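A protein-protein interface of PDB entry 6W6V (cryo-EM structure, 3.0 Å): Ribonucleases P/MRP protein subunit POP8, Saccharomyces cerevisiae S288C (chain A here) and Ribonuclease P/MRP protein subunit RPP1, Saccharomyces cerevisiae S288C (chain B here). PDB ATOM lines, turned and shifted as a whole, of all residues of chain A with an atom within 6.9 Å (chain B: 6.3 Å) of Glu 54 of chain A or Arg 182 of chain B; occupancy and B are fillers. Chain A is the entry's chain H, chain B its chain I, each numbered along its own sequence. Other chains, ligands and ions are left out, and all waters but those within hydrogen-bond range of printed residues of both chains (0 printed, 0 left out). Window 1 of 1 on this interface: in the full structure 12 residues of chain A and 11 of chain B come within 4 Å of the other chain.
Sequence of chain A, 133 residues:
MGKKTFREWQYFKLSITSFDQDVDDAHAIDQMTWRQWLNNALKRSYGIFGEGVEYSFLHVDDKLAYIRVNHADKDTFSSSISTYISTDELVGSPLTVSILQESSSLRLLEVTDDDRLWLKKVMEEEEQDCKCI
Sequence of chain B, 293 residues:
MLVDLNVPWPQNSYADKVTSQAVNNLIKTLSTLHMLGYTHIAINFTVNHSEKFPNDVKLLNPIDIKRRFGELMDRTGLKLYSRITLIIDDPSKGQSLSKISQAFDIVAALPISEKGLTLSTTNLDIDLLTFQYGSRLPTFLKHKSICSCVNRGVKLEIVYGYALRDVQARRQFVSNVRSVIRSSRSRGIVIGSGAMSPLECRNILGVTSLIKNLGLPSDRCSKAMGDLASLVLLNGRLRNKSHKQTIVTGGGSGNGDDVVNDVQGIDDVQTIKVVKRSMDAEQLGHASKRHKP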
ATOM      1  N   PHE A   6       9.477  22.110 -42.713  1.00  0.00           N
ATOM      2  CA  PHE A   6      10.051  22.485 -41.430  1.00  0.00           C
ATOM      3  C   PHE A   6      11.340  21.707 -41.228  1.00  0.00           C
ATOM      4  O   PHE A   6      11.412  20.519 -41.555  1.00  0.00           O
ATOM      5  CB  PHE A   6       9.076  22.212 -40.281  1.00  0.00           C
ATOM      6  CG  PHE A   6       9.601  22.612 -38.935  1.00  0.00           C
ATOM      7  CD1 PHE A   6       9.435  23.904 -38.472  1.00  0.00           C
ATOM      8  CD2 PHE A   6      10.254  21.697 -38.130  1.00  0.00           C
ATOM      9  CE1 PHE A   6       9.913  24.275 -37.235  1.00  0.00           C
ATOM     10  CE2 PHE A   6      10.737  22.065 -36.894  1.00  0.00           C
ATOM     11  CZ  PHE A   6      10.565  23.353 -36.444  1.00  0.00           C
ATOM     12  N   GLU A   8      14.423  20.847 -38.327  1.00  0.00           N
ATOM     13  CA  GLU A   8      14.711  20.848 -36.899  1.00  0.00           C
ATOM     14  C   GLU A   8      16.200  20.809 -36.592  1.00  0.00           C
ATOM     15  O   GLU A   8      16.688  21.604 -35.786  1.00  0.00           O
ATOM     16  CB  GLU A   8      14.019  19.661 -36.221  1.00  0.00           C
ATOM     17  CG  GLU A   8      14.200  19.626 -34.716  1.00  0.00           C
ATOM     18  CD  GLU A   8      13.464  18.474 -34.064  1.00  0.00           C
ATOM     19  OE1 GLU A   8      12.826  17.685 -34.790  1.00  0.00           O
ATOM     20  OE2 GLU A   8      13.517  18.359 -32.823  1.00  0.00           O
ATOM     21  N   TRP A   9      16.934  19.898 -37.219  1.00  0.00           N
ATOM     22  CA  TRP A   9      18.325  19.658 -36.884  1.00  0.00           C
ATOM     23  C   TRP A   9      19.224  19.995 -38.065  1.00  0.00           C
ATOM     24  O   TRP A   9      18.780  20.074 -39.212  1.00  0.00           O
ATOM     25  CB  TRP A   9      18.538  18.199 -36.465  1.00  0.00           C
ATOM     26  CG  TRP A   9      17.878  17.847 -35.172  1.00  0.00           C
ATOM     27  CD1 TRP A   9      16.757  17.090 -35.005  1.00  0.00           C
ATOM     28  CD2 TRP A   9      18.307  18.224 -33.860  1.00  0.00           C
ATOM     29  NE1 TRP A   9      16.456  16.980 -33.671  1.00  0.00           N
ATOM     30  CE2 TRP A   9      17.394  17.668 -32.946  1.00  0.00           C
ATOM     31  CE3 TRP A   9      19.374  18.984 -33.369  1.00  0.00           C
ATOM     32  CZ2 TRP A   9      17.514  17.845 -31.573  1.00  0.00           C
ATOM     33  CZ3 TRP A   9      19.489  19.158 -32.006  1.00  0.00           C
ATOM     34  CH2 TRP A   9      18.566  18.591 -31.123  1.00  0.00           C
ATOM     35  N   GLU A  51      25.825  30.161 -24.481  1.00  0.00           N
ATOM     36  CA  GLU A  51      25.982  28.899 -23.775  1.00  0.00           C
ATOM     37  C   GLU A  51      24.827  27.947 -24.006  1.00  0.00           C
ATOM     38  O   GLU A  51      25.011  26.730 -23.913  1.00  0.00           O
ATOM     39  CB  GLU A  51      26.113  29.147 -22.271  1.00  0.00           C
ATOM     40  CG  GLU A  51      27.363  29.887 -21.887  1.00  0.00           C
ATOM     41  CD  GLU A  51      28.601  29.077 -22.150  1.00  0.00           C
ATOM     42  OE1 GLU A  51      28.531  27.836 -22.045  1.00  0.00           O
ATOM     43  OE2 GLU A  51      29.641  29.682 -22.465  1.00  0.00           O
ATOM     44  N   GLY A  52      23.649  28.471 -24.313  1.00  0.00           N
ATOM     45  CA  GLY A  52      22.456  27.670 -24.432  1.00  0.00           C
ATOM     46  C   GLY A  52      22.308  26.906 -25.719  1.00  0.00           C
ATOM     47  O   GLY A  52      21.300  26.218 -25.897  1.00  0.00           O
ATOM     48  N   VAL A  53      23.270  27.006 -26.635  1.00  0.00           N
ATOM     49  CA  VAL A  53      23.226  26.207 -27.851  1.00  0.00           C
ATOM     50  C   VAL A  53      23.285  24.738 -27.454  1.00  0.00           C
ATOM     51  O   VAL A  53      24.280  24.274 -26.888  1.00  0.00           O
ATOM     52  CB  VAL A  53      24.361  26.584 -28.819  1.00  0.00           C
ATOM     53  CG1 VAL A  53      24.066  27.910 -29.478  1.00  0.00           C
ATOM     54  CG2 VAL A  53      25.676  26.673 -28.084  1.00  0.00           C
ATOM     55  N   GLU A  54      22.210  24.004 -27.719  1.00  0.00           N
ATOM     56  CA  GLU A  54      22.146  22.594 -27.366  1.00  0.00           C
ATOM     57  C   GLU A  54      22.579  21.760 -28.564  1.00  0.00           C
ATOM     58  O   GLU A  54      21.975  21.835 -29.638  1.00  0.00           O
ATOM     59  CB  GLU A  54      20.745  22.201 -26.901  1.00  0.00           C
ATOM     60  CG  GLU A  54      19.624  22.608 -27.827  1.00  0.00           C
ATOM     61  CD  GLU A  54      18.303  21.979 -27.439  1.00  0.00           C
ATOM     62  OE1 GLU A  54      17.418  21.861 -28.312  1.00  0.00           O
ATOM     63  OE2 GLU A  54      18.155  21.591 -26.263  1.00  0.00           O
ATOM     64  N   TYR A  55      23.630  20.974 -28.375  1.00  0.00           N
ATOM     65  CA  TYR A  55      24.193  20.142 -29.421  1.00  0.00           C
ATOM     66  C   TYR A  55      24.381  18.729 -28.893  1.00  0.00           C
ATOM     67  O   TYR A  55      24.614  18.520 -27.701  1.00  0.00           O
ATOM     68  CB  TYR A  55      25.511  20.739 -29.938  1.00  0.00           C
ATOM     69  CG  TYR A  55      26.596  20.883 -28.896  1.00  0.00           C
ATOM     70  CD1 TYR A  55      27.012  22.136 -28.487  1.00  0.00           C
ATOM     71  CD2 TYR A  55      27.234  19.780 -28.360  1.00  0.00           C
ATOM     72  CE1 TYR A  55      27.999  22.285 -27.548  1.00  0.00           C
ATOM     73  CE2 TYR A  55      28.222  19.919 -27.421  1.00  0.00           C
ATOM     74  CZ  TYR A  55      28.604  21.173 -27.020  1.00  0.00           C
ATOM     75  OH  TYR A  55      29.597  21.312 -26.082  1.00  0.00           O
ATOM     76  N   SER A  56      24.254  17.760 -29.789  1.00  0.00           N
ATOM     77  CA  SER A  56      24.350  16.352 -29.433  1.00  0.00           C
ATOM     78  C   SER A  56      25.490  15.709 -30.203  1.00  0.00           C
ATOM     79  O   SER A  56      25.611  15.903 -31.419  1.00  0.00           O
ATOM     80  CB  SER A  56      23.039  15.619 -29.721  1.00  0.00           C
ATOM     81  OG  SER A  56      21.970  16.175 -28.977  1.00  0.00           O
ATOM     82  N   ARG A  68      25.136  17.189 -34.037  1.00  0.00           N
ATOM     83  CA  ARG A  68      23.870  17.745 -34.491  1.00  0.00           C
ATOM     84  C   ARG A  68      23.511  18.946 -33.626  1.00  0.00           C
ATOM     85  O   ARG A  68      23.720  18.932 -32.409  1.00  0.00           O
ATOM     86  CB  ARG A  68      22.749  16.707 -34.464  1.00  0.00           C
ATOM     87  CG  ARG A  68      22.288  16.292 -33.093  1.00  0.00           C
ATOM     88  CD  ARG A  68      21.271  15.181 -33.196  1.00  0.00           C
ATOM     89  NE  ARG A  68      20.566  14.959 -31.941  1.00  0.00           N
ATOM     90  CZ  ARG A  68      19.575  14.088 -31.794  1.00  0.00           C
ATOM     91  NH1 ARG A  68      19.177  13.358 -32.825  1.00  0.00           N
ATOM     92  NH2 ARG A  68      18.983  13.947 -30.618  1.00  0.00           N
ATOM     93  N   VAL A  69      22.996  19.995 -34.272  1.00  0.00           N
ATOM     94  CA  VAL A  69      22.704  21.272 -33.633  1.00  0.00           C
ATOM     95  C   VAL A  69      21.306  21.701 -34.067  1.00  0.00           C
ATOM     96  O   VAL A  69      20.780  21.231 -35.076  1.00  0.00           O
ATOM     97  CB  VAL A  69      23.764  22.342 -34.003  1.00  0.00           C
ATOM     98  CG1 VAL A  69      23.465  23.689 -33.373  1.00  0.00           C
ATOM     99  CG2 VAL A  69      25.150  21.876 -33.604  1.00  0.00           C
ATOM    100  N   ASN A  70      20.688  22.580 -33.276  1.00  0.00           N
ATOM    101  CA  ASN A  70      19.395  23.134 -33.658  1.00  0.00           C
ATOM    102  C   ASN A  70      19.497  23.848 -35.001  1.00  0.00           C
ATOM    103  O   ASN A  70      20.572  24.266 -35.436  1.00  0.00           O
ATOM    104  CB  ASN A  70      18.884  24.130 -32.618  1.00  0.00           C
ATOM    105  CG  ASN A  70      19.077  23.651 -31.207  1.00  0.00           C
ATOM    106  OD1 ASN A  70      19.642  24.358 -30.378  1.00  0.00           O
ATOM    107  ND2 ASN A  70      18.608  22.448 -30.922  1.00  0.00           N
ATOM    108  N   ASP A  73      20.549  27.675 -34.517  1.00  0.00           N
ATOM    109  CA  ASP A  73      21.863  27.996 -33.979  1.00  0.00           C
ATOM    110  C   ASP A  73      22.976  27.805 -34.998  1.00  0.00           C
ATOM    111  O   ASP A  73      24.150  27.991 -34.659  1.00  0.00           O
ATOM    112  CB  ASP A  73      22.138  27.159 -32.731  1.00  0.00           C
ATOM    113  CG  ASP A  73      21.140  27.425 -31.627  1.00  0.00           C
ATOM    114  OD1 ASP A  73      20.220  28.238 -31.846  1.00  0.00           O
ATOM    115  OD2 ASP A  73      21.268  26.819 -30.545  1.00  0.00           O
ATOM    116  N   PHE B 140      16.712  16.032 -22.805  1.00  0.00           N
ATOM    117  CA  PHE B 140      16.236  15.251 -23.942  1.00  0.00           C
ATOM    118  C   PHE B 140      14.724  15.044 -23.841  1.00  0.00           C
ATOM    119  O   PHE B 140      14.217  13.937 -23.657  1.00  0.00           O
ATOM    120  CB  PHE B 140      16.997  13.928 -24.063  1.00  0.00           C
ATOM    121  CG  PHE B 140      16.589  13.096 -25.250  1.00  0.00           C
ATOM    122  CD1 PHE B 140      17.009  13.445 -26.523  1.00  0.00           C
ATOM    123  CD2 PHE B 140      15.827  11.951 -25.093  1.00  0.00           C
ATOM    124  CE1 PHE B 140      16.650  12.688 -27.620  1.00  0.00           C
ATOM    125  CE2 PHE B 140      15.464  11.188 -26.188  1.00  0.00           C
ATOM    126  CZ  PHE B 140      15.878  11.557 -27.453  1.00  0.00           C
ATOM    127  N   LEU B 141      14.010  16.160 -23.922  1.00  0.00           N
ATOM    128  CA  LEU B 141      12.561  16.162 -24.046  1.00  0.00           C
ATOM    129  C   LEU B 141      12.207  16.497 -25.488  1.00  0.00           C
ATOM    130  O   LEU B 141      12.740  17.456 -26.056  1.00  0.00           O
ATOM    131  CB  LEU B 141      11.921  17.153 -23.069  1.00  0.00           C
ATOM    132  CG  LEU B 141      12.026  18.665 -23.288  1.00  0.00           C
ATOM    133  CD1 LEU B 141      11.011  19.386 -22.424  1.00  0.00           C
ATOM    134  CD2 LEU B 141      13.426  19.171 -22.984  1.00  0.00           C
ATOM    135  N   LYS B 142      11.336  15.693 -26.084  1.00  0.00           N
ATOM    136  CA  LYS B 142      11.092  15.750 -27.516  1.00  0.00           C
ATOM    137  C   LYS B 142       9.624  16.026 -27.803  1.00  0.00           C
ATOM    138  O   LYS B 142       8.778  16.047 -26.908  1.00  0.00           O
ATOM    139  CB  LYS B 142      11.530  14.448 -28.198  1.00  0.00           C
ATOM    140  CG  LYS B 142      10.944  13.194 -27.580  1.00  0.00           C
ATOM    141  CD  LYS B 142      11.869  12.006 -27.783  1.00  0.00           C
ATOM    142  CE  LYS B 142      11.313  10.749 -27.134  1.00  0.00           C
ATOM    143  NZ  LYS B 142      10.850  10.998 -25.742  1.00  0.00           N
ATOM    144  N   HIS B 143       9.339  16.228 -29.091  1.00  0.00           N
ATOM    145  CA  HIS B 143       7.989  16.543 -29.538  1.00  0.00           C
ATOM    146  C   HIS B 143       6.995  15.448 -29.176  1.00  0.00           C
ATOM    147  O   HIS B 143       5.792  15.721 -29.090  1.00  0.00           O
ATOM    148  CB  HIS B 143       8.010  16.785 -31.050  1.00  0.00           C
ATOM    149  CG  HIS B 143       6.664  17.043 -31.655  1.00  0.00           C
ATOM    150  ND1 HIS B 143       6.134  18.308 -31.780  1.00  0.00           N
ATOM    151  CD2 HIS B 143       5.757  16.200 -32.204  1.00  0.00           C
ATOM    152  CE1 HIS B 143       4.951  18.233 -32.362  1.00  0.00           C
ATOM    153  NE2 HIS B 143       4.701  16.966 -32.633  1.00  0.00           N
ATOM    154  N   SER B 175      19.816  28.067 -21.155  1.00  0.00           N
ATOM    155  CA  SER B 175      19.987  26.766 -21.794  1.00  0.00           C
ATOM    156  C   SER B 175      18.657  26.033 -21.936  1.00  0.00           C
ATOM    157  O   SER B 175      18.368  25.462 -22.991  1.00  0.00           O
ATOM    158  CB  SER B 175      20.986  25.921 -21.006  1.00  0.00           C
ATOM    159  OG  SER B 175      21.380  24.780 -21.746  1.00  0.00           O
ATOM    160  N   VAL B 177      15.503  27.262 -21.843  1.00  0.00           N
ATOM    161  CA  VAL B 177      14.446  27.929 -22.593  1.00  0.00           C
ATOM    162  C   VAL B 177      14.551  27.598 -24.076  1.00  0.00           C
ATOM    163  O   VAL B 177      13.536  27.438 -24.760  1.00  0.00           O
ATOM    164  CB  VAL B 177      14.472  29.446 -22.334  1.00  0.00           C
ATOM    165  CG1 VAL B 177      15.756  30.055 -22.843  1.00  0.00           C
ATOM    166  CG2 VAL B 177      13.273  30.107 -22.974  1.00  0.00           C
ATOM    167  N   ARG B 178      15.774  27.469 -24.597  1.00  0.00           N
ATOM    168  CA  ARG B 178      15.933  27.101 -25.999  1.00  0.00           C
ATOM    169  C   ARG B 178      15.358  25.717 -26.270  1.00  0.00           C
ATOM    170  O   ARG B 178      14.666  25.506 -27.277  1.00  0.00           O
ATOM    171  CB  ARG B 178      17.407  27.162 -26.391  1.00  0.00           C
ATOM    172  CG  ARG B 178      17.877  28.542 -26.794  1.00  0.00           C
ATOM    173  CD  ARG B 178      19.334  28.523 -27.197  1.00  0.00           C
ATOM    174  NE  ARG B 178      19.748  29.772 -27.823  1.00  0.00           N
ATOM    175  CZ  ARG B 178      20.802  30.485 -27.442  1.00  0.00           C
ATOM    176  NH1 ARG B 178      21.109  31.609 -28.071  1.00  0.00           N
ATOM    177  NH2 ARG B 178      21.553  30.073 -26.434  1.00  0.00           N
ATOM    178  N   SER B 179      15.623  24.765 -25.374  1.00  0.00           N
ATOM    179  CA  SER B 179      15.085  23.420 -25.538  1.00  0.00           C
ATOM    180  C   SER B 179      13.564  23.433 -25.518  1.00  0.00           C
ATOM    181  O   SER B 179      12.915  22.811 -26.366  1.00  0.00           O
ATOM    182  CB  SER B 179      15.623  22.504 -24.442  1.00  0.00           C
ATOM    183  OG  SER B 179      17.027  22.372 -24.537  1.00  0.00           O
ATOM    184  N   VAL B 180      12.974  24.146 -24.557  1.00  0.00           N
ATOM    185  CA  VAL B 180      11.517  24.115 -24.469  1.00  0.00           C
ATOM    186  C   VAL B 180      10.884  24.831 -25.658  1.00  0.00           C
ATOM    187  O   VAL B 180       9.807  24.437 -26.120  1.00  0.00           O
ATOM    188  CB  VAL B 180      11.026  24.685 -23.124  1.00  0.00           C
ATOM    189  CG1 VAL B 180      11.438  26.121 -22.959  1.00  0.00           C
ATOM    190  CG2 VAL B 180       9.516  24.542 -23.007  1.00  0.00           C
ATOM    191  N   ILE B 181      11.526  25.878 -26.184  1.00  0.00           N
ATOM    192  CA  ILE B 181      10.997  26.528 -27.381  1.00  0.00           C
ATOM    193  C   ILE B 181      11.043  25.583 -28.570  1.00  0.00           C
ATOM    194  O   ILE B 181      10.039  25.384 -29.262  1.00  0.00           O
ATOM    195  CB  ILE B 181      11.747  27.836 -27.683  1.00  0.00           C
ATOM    196  CG1 ILE B 181      11.548  28.847 -26.559  1.00  0.00           C
ATOM    197  CG2 ILE B 181      11.285  28.412 -29.002  1.00  0.00           C
ATOM    198  CD1 ILE B 181      12.453  30.045 -26.664  1.00  0.00           C
ATOM    199  N   ARG B 182      12.202  24.971 -28.825  1.00  0.00           N
ATOM    200  CA  ARG B 182      12.319  24.191 -30.051  1.00  0.00           C
ATOM    201  C   ARG B 182      11.583  22.861 -29.968  1.00  0.00           C
ATOM    202  O   ARG B 182      11.298  22.264 -31.010  1.00  0.00           O
ATOM    203  CB  ARG B 182      13.789  23.953 -30.415  1.00  0.00           C
ATOM    204  CG  ARG B 182      14.580  23.114 -29.436  1.00  0.00           C
ATOM    205  CD  ARG B 182      14.512  21.638 -29.795  1.00  0.00           C
ATOM    206  NE  ARG B 182      15.334  20.824 -28.914  1.00  0.00           N
ATOM    207  CZ  ARG B 182      15.292  19.500 -28.886  1.00  0.00           C
ATOM    208  NH1 ARG B 182      16.069  18.829 -28.053  1.00  0.00           N
ATOM    209  NH2 ARG B 182      14.463  18.849 -29.687  1.00  0.00           N
ATOM    210  N   SER B 183      11.277  22.377 -28.765  1.00  0.00           N
ATOM    211  CA  SER B 183      10.550  21.119 -28.658  1.00  0.00           C
ATOM    212  C   SER B 183       9.077  21.273 -29.006  1.00  0.00           C
ATOM    213  O   SER B 183       8.468  20.334 -29.524  1.00  0.00           O
ATOM    214  CB  SER B 183      10.686  20.548 -27.251  1.00  0.00           C
ATOM    215  OG  SER B 183       9.797  21.200 -26.366  1.00  0.00           O
ATOM    216  N   SER B 184       8.489  22.432 -28.729  1.00  0.00           N
ATOM    217  CA  SER B 184       7.074  22.661 -28.977  1.00  0.00           C
ATOM    218  C   SER B 184       6.799  23.329 -30.314  1.00  0.00           C
ATOM    219  O   SER B 184       5.638  23.623 -30.612  1.00  0.00           O
ATOM    220  CB  SER B 184       6.470  23.509 -27.857  1.00  0.00           C
ATOM    221  OG  SER B 184       5.252  24.099 -28.277  1.00  0.00           O
ATOM    222  N   ARG B 185       7.833  23.581 -31.116  1.00  0.00           N
ATOM    223  CA  ARG B 185       7.680  24.214 -32.427  1.00  0.00           C
ATOM    224  C   ARG B 185       6.982  25.567 -32.315  1.00  0.00           C
ATOM    225  O   ARG B 185       6.186  25.945 -33.177  1.00  0.00           O
ATOM    226  CB  ARG B 185       6.937  23.299 -33.401  1.00  0.00           C
ATOM    227  CG  ARG B 185       7.413  21.857 -33.395  1.00  0.00           C
ATOM    228  CD  ARG B 185       8.885  21.757 -33.746  1.00  0.00           C
ATOM    229  NE  ARG B 185       9.160  20.632 -34.633  1.00  0.00           N
ATOM    230  CZ  ARG B 185       9.811  19.533 -34.271  1.00  0.00           C
ATOM    231  NH1 ARG B 185      10.262  19.404 -33.033  1.00  0.00           N
ATOM    232  NH2 ARG B 185      10.014  18.562 -35.149  1.00  0.00           N
ATOM    233  N   SER B 186       7.277  26.295 -31.238  1.00  0.00           N
ATOM    234  CA  SER B 186       6.788  27.660 -31.037  1.00  0.00           C
ATOM    235  C   SER B 186       5.262  27.723 -31.049  1.00  0.00           C
ATOM    236  O   SER B 186       4.658  28.546 -31.737  1.00  0.00           O
ATOM    237  CB  SER B 186       7.381  28.607 -32.081  1.00  0.00           C
ATOM    238  OG  SER B 186       8.789  28.680 -31.962  1.00  0.00           O
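OE1 of Glu 54 of chain A is in salt-bridge range of NE of Arg 182 of chain B (2.4 Å).
The side-chain carboxylate (OE2) of Glu 8 of chain A lies within salt-bridge range of the guanidinium group (NH2) of Arg 182 of chain B (3.3 Å).
The side-chain carboxylate (OE2) of Glu 54 of chain A lies close to the side-chain hydroxyl (OG) of Ser 179 of chain B (2.2 Å).
NH2 of Arg 178 of chain B lies close to N of Gly 52 of chain A.
NH2 of Arg 185 of chain B lies within salt-bridge range of OE1 of Glu 8 of chain A (3.0 Å).
OE1 of Glu 54 of chain A lies within hydrogen-bond range of ND2 of Asn 70 of chain A, at 2.9 Å.
The side-chain carboxylate (OE2) of Glu 8 of chain A lies within hydrogen-bond range of the indole nitrogen (NE1) of Trp 9 of chain A, at 3.4 Å.
Among the printed residues, pairs that only touch across the chains: Phe 6 of chain A with Arg 185 of chain B (3.1 Å), Trp 9 of chain A with Arg 182 of chain B (3.7 Å), Gly 52 of chain A with Ser 175 of chain B (3.7 Å) and Val 53 of chain A with Arg 178 of chain B (3.5 Å).
Printed residues of chain B within 4 Å of Phe 6 of chain A: Arg 185 (3.1 Å).
Printed residues of chain B within 4 Å of Gly 52 of chain A: Ser 175 and Arg 178.
Of the printed residues of chain B, Val 53 of chain A touches Arg 178 (3.5 Å).
Of chain B, only Ser 179 and Arg 182 come within 4 Å of Glu 54 of chain A.
Of the printed residues of chain A, Ser 175 of chain B touches Gly 52.
Printed residues of chain A within 4 Å of Arg 178 of chain B: Gly 52 (3.3 Å) and Val 53 (3.5 Å).
Val 180 of chain B touches none of the printed residues of chain A.
Arg 182 of chain B touches three residues of chain A.
The nearest residue of chain B that does not touch Glu 54 of chain A is Arg 178 of chain B (4.7 Å).
Among the printed residues, Asp or Glu carboxylates within 4 Å of a Lys or Arg side-chain nitrogen of the other chain: Glu 8 of chain A with Arg 182 of chain B, Glu 8 of chain A with Arg 185 of chain B and Glu 54 of chain A with Arg 182 of chain B.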
